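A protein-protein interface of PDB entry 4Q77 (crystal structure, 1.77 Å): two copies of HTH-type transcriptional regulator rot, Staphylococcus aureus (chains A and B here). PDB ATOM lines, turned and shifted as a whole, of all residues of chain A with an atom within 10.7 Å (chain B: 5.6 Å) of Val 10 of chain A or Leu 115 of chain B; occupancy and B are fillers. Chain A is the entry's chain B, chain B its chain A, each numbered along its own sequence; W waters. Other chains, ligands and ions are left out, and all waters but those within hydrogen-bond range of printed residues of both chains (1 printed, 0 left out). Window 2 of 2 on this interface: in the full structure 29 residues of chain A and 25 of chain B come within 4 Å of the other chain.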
ATOM      1  N   VAL A  10      29.770  -3.520  20.166  1.00  0.00           N
ATOM      2  CA  VAL A  10      28.596  -3.028  19.383  1.00  0.00           C
ATOM      3  C   VAL A  10      28.485  -1.500  19.438  1.00  0.00           C
ATOM      4  O   VAL A  10      28.556  -0.910  20.521  1.00  0.00           O
ATOM      5  CB  VAL A  10      27.280  -3.630  19.913  1.00  0.00           C
ATOM      6  N   ASN A  11      28.324  -0.870  18.275  1.00  0.00           N
ATOM      7  CA  ASN A  11      28.148   0.591  18.178  1.00  0.00           C
ATOM      8  C   ASN A  11      27.248   0.956  16.982  1.00  0.00           C
ATOM      9  O   ASN A  11      26.575   0.077  16.426  1.00  0.00           O
ATOM     10  CB  ASN A  11      29.519   1.295  18.111  1.00  0.00           C
ATOM     11  CG  ASN A  11      30.463   0.661  17.091  1.00  0.00           C
ATOM     12  OD1 ASN A  11      30.146   0.583  15.907  1.00  0.00           O
ATOM     13  ND2 ASN A  11      31.628   0.204  17.553  1.00  0.00           N
ATOM     14  N   ASN A  12      27.203   2.236  16.604  1.00  0.00           N
ATOM     15  CA  ASN A  12      26.451   2.656  15.415  1.00  0.00           C
ATOM     16  C   ASN A  12      26.918   1.914  14.173  1.00  0.00           C
ATOM     17  O   ASN A  12      26.100   1.498  13.349  1.00  0.00           O
ATOM     18  CB  ASN A  12      26.583   4.160  15.172  1.00  0.00           C
ATOM     19  N   ASP A  13      28.235   1.742  14.058  1.00  0.00           N
ATOM     20  CA  ASP A  13      28.825   1.066  12.906  1.00  0.00           C
ATOM     21  C   ASP A  13      28.443  -0.409  12.839  1.00  0.00           C
ATOM     22  O   ASP A  13      28.377  -0.967  11.757  1.00  0.00           O
ATOM     23  CB  ASP A  13      30.351   1.227  12.871  1.00  0.00           C
ATOM     24  CG  ASP A  13      30.789   2.648  12.547  1.00  0.00           C
ATOM     25  OD1 ASP A  13      29.932   3.456  12.112  1.00  0.00           O
ATOM     26  OD2 ASP A  13      31.994   2.955  12.725  1.00  0.00           O
ATOM     27  N   THR A  14      28.178  -1.037  13.982  1.00  0.00           N
ATOM     28  CA  THR A  14      27.740  -2.430  13.983  1.00  0.00           C
ATOM     29  C   THR A  14      26.401  -2.554  13.271  1.00  0.00           C
ATOM     30  O   THR A  14      26.232  -3.390  12.371  1.00  0.00           O
ATOM     31  CB  THR A  14      27.593  -2.967  15.417  1.00  0.00           C
ATOM     32  OG1 THR A  14      28.813  -2.739  16.127  1.00  0.00           O
ATOM     33  CG2 THR A  14      27.287  -4.451  15.416  1.00  0.00           C
ATOM     34  N   VAL A  15      25.457  -1.713  13.673  1.00  0.00           N
ATOM     35  CA  VAL A  15      24.109  -1.747  13.103  1.00  0.00           C
ATOM     36  C   VAL A  15      24.135  -1.351  11.620  1.00  0.00           C
ATOM     37  O   VAL A  15      23.503  -1.995  10.796  1.00  0.00           O
ATOM     38  CB  VAL A  15      23.141  -0.863  13.917  1.00  0.00           C
ATOM     39  CG1 VAL A  15      21.791  -0.754  13.231  1.00  0.00           C
ATOM     40  CG2 VAL A  15      22.978  -1.423  15.331  1.00  0.00           C
ATOM     41  N   PHE A  16      24.884  -0.308  11.279  1.00  0.00           N
ATOM     42  CA  PHE A  16      25.019   0.100   9.878  1.00  0.00           C
ATOM     43  C   PHE A  16      25.584  -1.027   9.007  1.00  0.00           C
ATOM     44  O   PHE A  16      25.084  -1.265   7.899  1.00  0.00           O
ATOM     45  CB  PHE A  16      25.912   1.330   9.754  1.00  0.00           C
ATOM     46  CG  PHE A  16      26.139   1.768   8.338  1.00  0.00           C
ATOM     47  CD1 PHE A  16      25.235   2.599   7.706  1.00  0.00           C
ATOM     48  CD2 PHE A  16      27.259   1.345   7.640  1.00  0.00           C
ATOM     49  CE1 PHE A  16      25.441   3.004   6.402  1.00  0.00           C
ATOM     50  CE2 PHE A  16      27.474   1.748   6.332  1.00  0.00           C
ATOM     51  CZ  PHE A  16      26.559   2.579   5.713  1.00  0.00           C
ATOM     52  N   GLY A  17      26.633  -1.689   9.505  1.00  0.00           N
ATOM     53  CA  GLY A  17      27.266  -2.798   8.813  1.00  0.00           C
ATOM     54  C   GLY A  17      26.326  -3.961   8.525  1.00  0.00           C
ATOM     55  O   GLY A  17      26.315  -4.518   7.420  1.00  0.00           O
ATOM     56  N   ILE A  18      25.541  -4.334   9.523  1.00  0.00           N
ATOM     57  CA  ILE A  18      24.556  -5.387   9.361  1.00  0.00           C
ATOM     58  C   ILE A  18      23.520  -4.990   8.308  1.00  0.00           C
ATOM     59  O   ILE A  18      23.181  -5.785   7.437  1.00  0.00           O
ATOM     60  CB  ILE A  18      23.896  -5.724  10.702  1.00  0.00           C
ATOM     61  CG1 ILE A  18      24.936  -6.337  11.643  1.00  0.00           C
ATOM     62  CG2 ILE A  18      22.730  -6.679  10.507  1.00  0.00           C
ATOM     63  CD1 ILE A  18      24.477  -6.394  13.093  1.00  0.00           C
ATOM     64  N   LEU A  19      23.040  -3.754   8.375  1.00  0.00           N
ATOM     65  CA  LEU A  19      22.068  -3.264   7.402  1.00  0.00           C
ATOM     66  C   LEU A  19      22.597  -3.301   5.964  1.00  0.00           C
ATOM     67  O   LEU A  19      21.815  -3.409   5.028  1.00  0.00           O
ATOM     68  CB  LEU A  19      21.567  -1.856   7.771  1.00  0.00           C
ATOM     69  CG  LEU A  19      20.545  -1.859   8.920  1.00  0.00           C
ATOM     70  CD1 LEU A  19      20.321  -0.471   9.498  1.00  0.00           C
ATOM     71  CD2 LEU A  19      19.215  -2.460   8.484  1.00  0.00           C
ATOM     72  N   LEU A  21      23.927  -5.742   4.584  1.00  0.00           N
ATOM     73  CA  LEU A  21      23.495  -6.997   3.966  1.00  0.00           C
ATOM     74  C   LEU A  21      22.360  -6.749   2.987  1.00  0.00           C
ATOM     75  O   LEU A  21      22.331  -7.333   1.902  1.00  0.00           O
ATOM     76  CB  LEU A  21      22.990  -7.988   5.006  1.00  0.00           C
ATOM     77  CG  LEU A  21      24.062  -8.583   5.910  1.00  0.00           C
ATOM     78  CD1 LEU A  21      23.400  -9.240   7.110  1.00  0.00           C
ATOM     79  CD2 LEU A  21      24.906  -9.580   5.131  1.00  0.00           C
ATOM     80  N   ALA A 135      31.797  -3.271   5.016  1.00  0.00           N
ATOM     81  CA  ALA A 135      31.011  -2.919   6.199  1.00  0.00           C
ATOM     82  C   ALA A 135      30.435  -4.162   6.870  1.00  0.00           C
ATOM     83  O   ALA A 135      30.502  -4.309   8.097  1.00  0.00           O
ATOM     84  CB  ALA A 135      29.893  -1.960   5.830  1.00  0.00           C
ATOM     85  N   ILE A 136      29.882  -5.053   6.060  1.00  0.00           N
ATOM     86  CA  ILE A 136      29.323  -6.319   6.548  1.00  0.00           C
ATOM     87  C   ILE A 136      30.359  -7.126   7.331  1.00  0.00           C
ATOM     88  O   ILE A 136      30.105  -7.562   8.451  1.00  0.00           O
ATOM     89  CB  ILE A 136      28.770  -7.158   5.382  1.00  0.00           C
ATOM     90  CG1 ILE A 136      27.519  -6.492   4.813  1.00  0.00           C
ATOM     91  CG2 ILE A 136      28.416  -8.575   5.832  1.00  0.00           C
ATOM     92  CD1 ILE A 136      27.208  -6.924   3.399  1.00  0.00           C
ATOM     93  N   ILE A 137      31.528  -7.296   6.737  1.00  0.00           N
ATOM     94  CA  ILE A 137      32.558  -8.174   7.282  1.00  0.00           C
ATOM     95  C   ILE A 137      33.199  -7.567   8.525  1.00  0.00           C
ATOM     96  O   ILE A 137      33.704  -8.297   9.376  1.00  0.00           O
ATOM     97  CB  ILE A 137      33.597  -8.546   6.201  1.00  0.00           C
ATOM     98  CG1 ILE A 137      32.950  -9.521   5.214  1.00  0.00           C
ATOM     99  CG2 ILE A 137      34.846  -9.167   6.811  1.00  0.00           C
ATOM    100  CD1 ILE A 137      33.807  -9.888   4.024  1.00  0.00           C
ATOM    101  N   ALA A 138      33.147  -6.243   8.642  1.00  0.00           N
ATOM    102  CA  ALA A 138      33.683  -5.544   9.805  1.00  0.00           C
ATOM    103  C   ALA A 138      32.755  -5.568  11.040  1.00  0.00           C
ATOM    104  O   ALA A 138      33.151  -5.102  12.120  1.00  0.00           O
ATOM    105  CB  ALA A 138      34.027  -4.105   9.429  1.00  0.00           C
ATOM    106  N   VAL A 139      31.543  -6.104  10.890  1.00  0.00           N
ATOM    107  CA  VAL A 139      30.584  -6.205  12.002  1.00  0.00           C
ATOM    108  C   VAL A 139      31.133  -7.059  13.167  1.00  0.00           C
ATOM    109  O   VAL A 139      30.962  -6.686  14.347  1.00  0.00           O
ATOM    110  CB  VAL A 139      29.240  -6.799  11.519  1.00  0.00           C
ATOM    111  CG1 VAL A 139      28.324  -7.113  12.687  1.00  0.00           C
ATOM    112  CG2 VAL A 139      28.532  -5.844  10.556  1.00  0.00           C
ATOM    113  N   LEU B  50      16.710  -3.270  13.617  1.00  0.00           N
ATOM    114  CA  LEU B  50      18.001  -2.660  13.279  1.00  0.00           C
ATOM    115  C   LEU B  50      17.845  -1.194  12.867  1.00  0.00           C
ATOM    116  O   LEU B  50      18.644  -0.342  13.242  1.00  0.00           O
ATOM    117  CB  LEU B  50      18.667  -3.432  12.134  1.00  0.00           C
ATOM    118  CG  LEU B  50      19.128  -4.861  12.414  1.00  0.00           C
ATOM    119  CD1 LEU B  50      19.451  -5.586  11.115  1.00  0.00           C
ATOM    120  CD2 LEU B  50      20.326  -4.865  13.350  1.00  0.00           C
ATOM    121  N   TRP B  53      17.264   0.927  15.980  1.00  0.00           N
ATOM    122  CA  TRP B  53      18.532   1.203  16.650  1.00  0.00           C
ATOM    123  C   TRP B  53      19.389   2.199  15.890  1.00  0.00           C
ATOM    124  O   TRP B  53      20.107   2.980  16.499  1.00  0.00           O
ATOM    125  CB  TRP B  53      19.311  -0.084  16.897  1.00  0.00           C
ATOM    126  CG  TRP B  53      18.591  -1.019  17.810  1.00  0.00           C
ATOM    127  CD1 TRP B  53      17.716  -0.682  18.796  1.00  0.00           C
ATOM    128  CD2 TRP B  53      18.686  -2.451  17.828  1.00  0.00           C
ATOM    129  NE1 TRP B  53      17.256  -1.814  19.430  1.00  0.00           N
ATOM    130  CE2 TRP B  53      17.838  -2.912  18.860  1.00  0.00           C
ATOM    131  CE3 TRP B  53      19.415  -3.386  17.090  1.00  0.00           C
ATOM    132  CZ2 TRP B  53      17.689  -4.267  19.161  1.00  0.00           C
ATOM    133  CZ3 TRP B  53      19.260  -4.741  17.393  1.00  0.00           C
ATOM    134  CH2 TRP B  53      18.402  -5.160  18.409  1.00  0.00           C
ATOM    135  N   GLU B 110      19.785  -8.011  25.603  1.00  0.00           N
ATOM    136  CA  GLU B 110      19.324  -8.821  24.479  1.00  0.00           C
ATOM    137  C   GLU B 110      19.753  -8.204  23.147  1.00  0.00           C
ATOM    138  O   GLU B 110      20.140  -8.932  22.246  1.00  0.00           O
ATOM    139  CB  GLU B 110      17.799  -9.059  24.508  1.00  0.00           C
ATOM    140  CG  GLU B 110      17.347 -10.207  25.413  1.00  0.00           C
ATOM    141  CD  GLU B 110      16.086 -10.914  24.918  1.00  0.00           C
ATOM    142  OE1 GLU B 110      16.061 -11.364  23.748  1.00  0.00           O
ATOM    143  OE2 GLU B 110      15.120 -11.040  25.706  1.00  0.00           O
ATOM    144  N   LYS B 111      19.704  -6.876  23.034  1.00  0.00           N
ATOM    145  CA  LYS B 111      20.184  -6.196  21.829  1.00  0.00           C
ATOM    146  C   LYS B 111      21.652  -6.537  21.565  1.00  0.00           C
ATOM    147  O   LYS B 111      22.020  -6.909  20.453  1.00  0.00           O
ATOM    148  CB  LYS B 111      19.989  -4.681  21.937  1.00  0.00           C
ATOM    149  CG  LYS B 111      20.791  -3.863  20.936  1.00  0.00           C
ATOM    150  CD  LYS B 111      20.560  -2.364  21.073  1.00  0.00           C
ATOM    151  CE  LYS B 111      21.464  -1.609  20.108  1.00  0.00           C
ATOM    152  NZ  LYS B 111      21.319  -0.135  20.229  1.00  0.00           N
ATOM    153  N   VAL B 112      22.477  -6.449  22.598  1.00  0.00           N
ATOM    154  CA  VAL B 112      23.901  -6.746  22.460  1.00  0.00           C
ATOM    155  C   VAL B 112      24.102  -8.192  22.032  1.00  0.00           C
ATOM    156  O   VAL B 112      24.921  -8.474  21.158  1.00  0.00           O
ATOM    157  CB  VAL B 112      24.672  -6.482  23.760  1.00  0.00           C
ATOM    158  CG1 VAL B 112      26.124  -6.944  23.636  1.00  0.00           C
ATOM    159  CG2 VAL B 112      24.621  -5.001  24.094  1.00  0.00           C
ATOM    160  N   GLU B 113      23.339  -9.097  22.641  1.00  0.00           N
ATOM    161  CA  GLU B 113      23.402 -10.525  22.313  1.00  0.00           C
ATOM    162  C   GLU B 113      22.988 -10.804  20.868  1.00  0.00           C
ATOM    163  O   GLU B 113      23.648 -11.589  20.179  1.00  0.00           O
ATOM    164  CB  GLU B 113      22.532 -11.339  23.279  1.00  0.00           C
ATOM    165  CG  GLU B 113      23.010 -12.769  23.475  1.00  0.00           C
ATOM    166  N   LEU B 114      21.911 -10.160  20.410  1.00  0.00           N
ATOM    167  CA  LEU B 114      21.477 -10.286  19.007  1.00  0.00           C
ATOM    168  C   LEU B 114      22.545  -9.800  18.041  1.00  0.00           C
ATOM    169  O   LEU B 114      22.843 -10.479  17.066  1.00  0.00           O
ATOM    170  CB  LEU B 114      20.162  -9.546  18.749  1.00  0.00           C
ATOM    171  CG  LEU B 114      19.639  -9.510  17.308  1.00  0.00           C
ATOM    172  CD1 LEU B 114      19.519 -10.894  16.705  1.00  0.00           C
ATOM    173  CD2 LEU B 114      18.275  -8.852  17.280  1.00  0.00           C
ATOM    174  N   LEU B 115      23.121  -8.636  18.309  1.00  0.00           N
ATOM    175  CA  LEU B 115      24.172  -8.098  17.442  1.00  0.00           C
ATOM    176  C   LEU B 115      25.395  -9.021  17.394  1.00  0.00           C
ATOM    177  O   LEU B 115      25.972  -9.210  16.329  1.00  0.00           O
ATOM    178  CB  LEU B 115      24.569  -6.679  17.858  1.00  0.00           C
ATOM    179  CG  LEU B 115      23.456  -5.625  17.741  1.00  0.00           C
ATOM    180  CD1 LEU B 115      23.873  -4.279  18.325  1.00  0.00           C
ATOM    181  CD2 LEU B 115      23.023  -5.454  16.295  1.00  0.00           C
ATOM    182  N   ASN B 116      25.770  -9.603  18.537  1.00  0.00           N
ATOM    183  CA  ASN B 116      26.854 -10.585  18.569  1.00  0.00           C
ATOM    184  C   ASN B 116      26.504 -11.842  17.783  1.00  0.00           C
ATOM    185  O   ASN B 116      27.359 -12.394  17.104  1.00  0.00           O
ATOM    186  CB  ASN B 116      27.223 -10.982  20.009  1.00  0.00           C
ATOM    187  CG  ASN B 116      27.922  -9.871  20.775  1.00  0.00           C
ATOM    188  OD1 ASN B 116      28.609  -9.024  20.199  1.00  0.00           O
ATOM    189  ND2 ASN B 116      27.764  -9.884  22.093  1.00  0.00           N
ATOM    190  N   PHE B 117      25.258 -12.308  17.893  1.00  0.00           N
ATOM    191  CA  PHE B 117      24.822 -13.476  17.135  1.00  0.00           C
ATOM    192  C   PHE B 117      24.962 -13.197  15.649  1.00  0.00           C
ATOM    193  O   PHE B 117      25.494 -14.019  14.906  1.00  0.00           O
ATOM    194  CB  PHE B 117      23.370 -13.830  17.445  1.00  0.00           C
ATOM    195  CG  PHE B 117      22.884 -15.082  16.753  1.00  0.00           C
ATOM    196  CD1 PHE B 117      23.046 -16.336  17.346  1.00  0.00           C
ATOM    197  CD2 PHE B 117      22.250 -15.012  15.518  1.00  0.00           C
ATOM    198  CE1 PHE B 117      22.590 -17.484  16.723  1.00  0.00           C
ATOM    199  CE2 PHE B 117      21.790 -16.161  14.884  1.00  0.00           C
ATOM    200  CZ  PHE B 117      21.960 -17.401  15.485  1.00  0.00           C
ATOM    201  N   ILE B 118      24.474 -12.033  15.220  1.00  0.00           N
ATOM    202  CA  ILE B 118      24.594 -11.641  13.819  1.00  0.00           C
ATOM    203  C   ILE B 118      26.053 -11.539  13.416  1.00  0.00           C
ATOM    204  O   ILE B 118      26.421 -12.042  12.358  1.00  0.00           O
ATOM    205  CB  ILE B 118      23.859 -10.326  13.509  1.00  0.00           C
ATOM    206  CG1 ILE B 118      22.368 -10.494  13.805  1.00  0.00           C
ATOM    207  CG2 ILE B 118      24.020  -9.952  12.042  1.00  0.00           C
ATOM    208  CD1 ILE B 118      21.538  -9.267  13.524  1.00  0.00           C
ATOM    209  N   SER B 119      26.881 -10.935  14.266  1.00  0.00           N
ATOM    210  CA  SER B 119      28.313 -10.819  13.991  1.00  0.00           C
ATOM    211  C   SER B 119      28.949 -12.195  13.737  1.00  0.00           C
ATOM    212  O   SER B 119      29.719 -12.392  12.781  1.00  0.00           O
ATOM    213  CB  SER B 119      29.017 -10.109  15.143  1.00  0.00           C
ATOM    214  OG  SER B 119      30.384  -9.887  14.841  1.00  0.00           O
ATOM    215  N   ASP B 120      28.597 -13.158  14.578  1.00  0.00           N
ATOM    216  CA  ASP B 120      29.091 -14.522  14.413  1.00  0.00           C
ATOM    217  C   ASP B 120      28.610 -15.204  13.120  1.00  0.00           C
ATOM    218  O   ASP B 120      29.359 -15.939  12.482  1.00  0.00           O
ATOM    219  CB  ASP B 120      28.671 -15.375  15.597  1.00  0.00           C
ATOM    220  CG  ASP B 120      29.361 -14.977  16.888  1.00  0.00           C
ATOM    221  OD1 ASP B 120      30.361 -14.218  16.877  1.00  0.00           O
ATOM    222  OD2 ASP B 120      28.894 -15.455  17.928  1.00  0.00           O
HETATM  223  O   HOH W   1      31.493  -7.740  16.485  1.00  0.00           O
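The side-chain hydroxyl (OG) of Ser 119 of chain B sits at hydrogen-bond distance from the backbone carbonyl oxygen (O) of Val 139 of chain A, at 3.3 Å.
Among the printed residues, pairs that only touch across the chains: Val 15 of chain A with Leu 50 of chain B (3.2 Å), Ile 18 of chain A with Leu 50 of chain B (3.5 Å), Ile 18 of chain A with Leu 115 of chain B (3.6 Å), Ile 18 of chain A with Ile 118 of chain B (3.7 Å), Val 10 of chain A with Leu 115 of chain B (3.8 Å) and Leu 19 of chain A with Leu 50 of chain B (3.8 Å).
Val 10 of chain A touches just one residue of chain B: Leu 115. Printed residues of chain B within 4 Å of Val 15 of chain A: Leu 50 (3.2 Å). Of the printed residues of chain A, Leu 50 of chain B touches Val 15 (3.2 Å), Ile 18 (3.5 Å) and Leu 19 (3.8 Å). No residue of chain A comes within 4 Å of Lys 111 of chain B. Leu 115 of chain B touches two residues of chain A. No residue of chain A comes within 4 Å of Asn 116 of chain B. Printed residues of chain A within 4 Å of Ser 119 of chain B: Val 139. The nearest residue of chain B that does not touch Val 10 of chain A is Val 112 of chain B (5.1 Å).
Hydrophobic or aromatic side chains of chain A within 4 Å of the printed part of chain B: Val 10, Val 15, Ile 18, Leu 19 and Val 139. Of the 13 printed residues of chain B, 4 touch a printed residue of chain A. Printed residues of chain B that touch a printed residue of chain A: Leu 50, Leu 115, Ile 118 and Ser 119. Hydrophobic or aromatic side chains of chain B that line the printed part of chain A: Leu 50, Leu 115 and Ile 118. Among the printed residues, 7 pairs touch across the chains.
No position is printed for both chains. Of the 7 pairs that touch across the chains among the printed residues, none has its exchanged pair printed and touching as well.
Water W1 lies within hydrogen-bond range of O of Val 139 of chain A and OG of Ser 119 of chain B.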
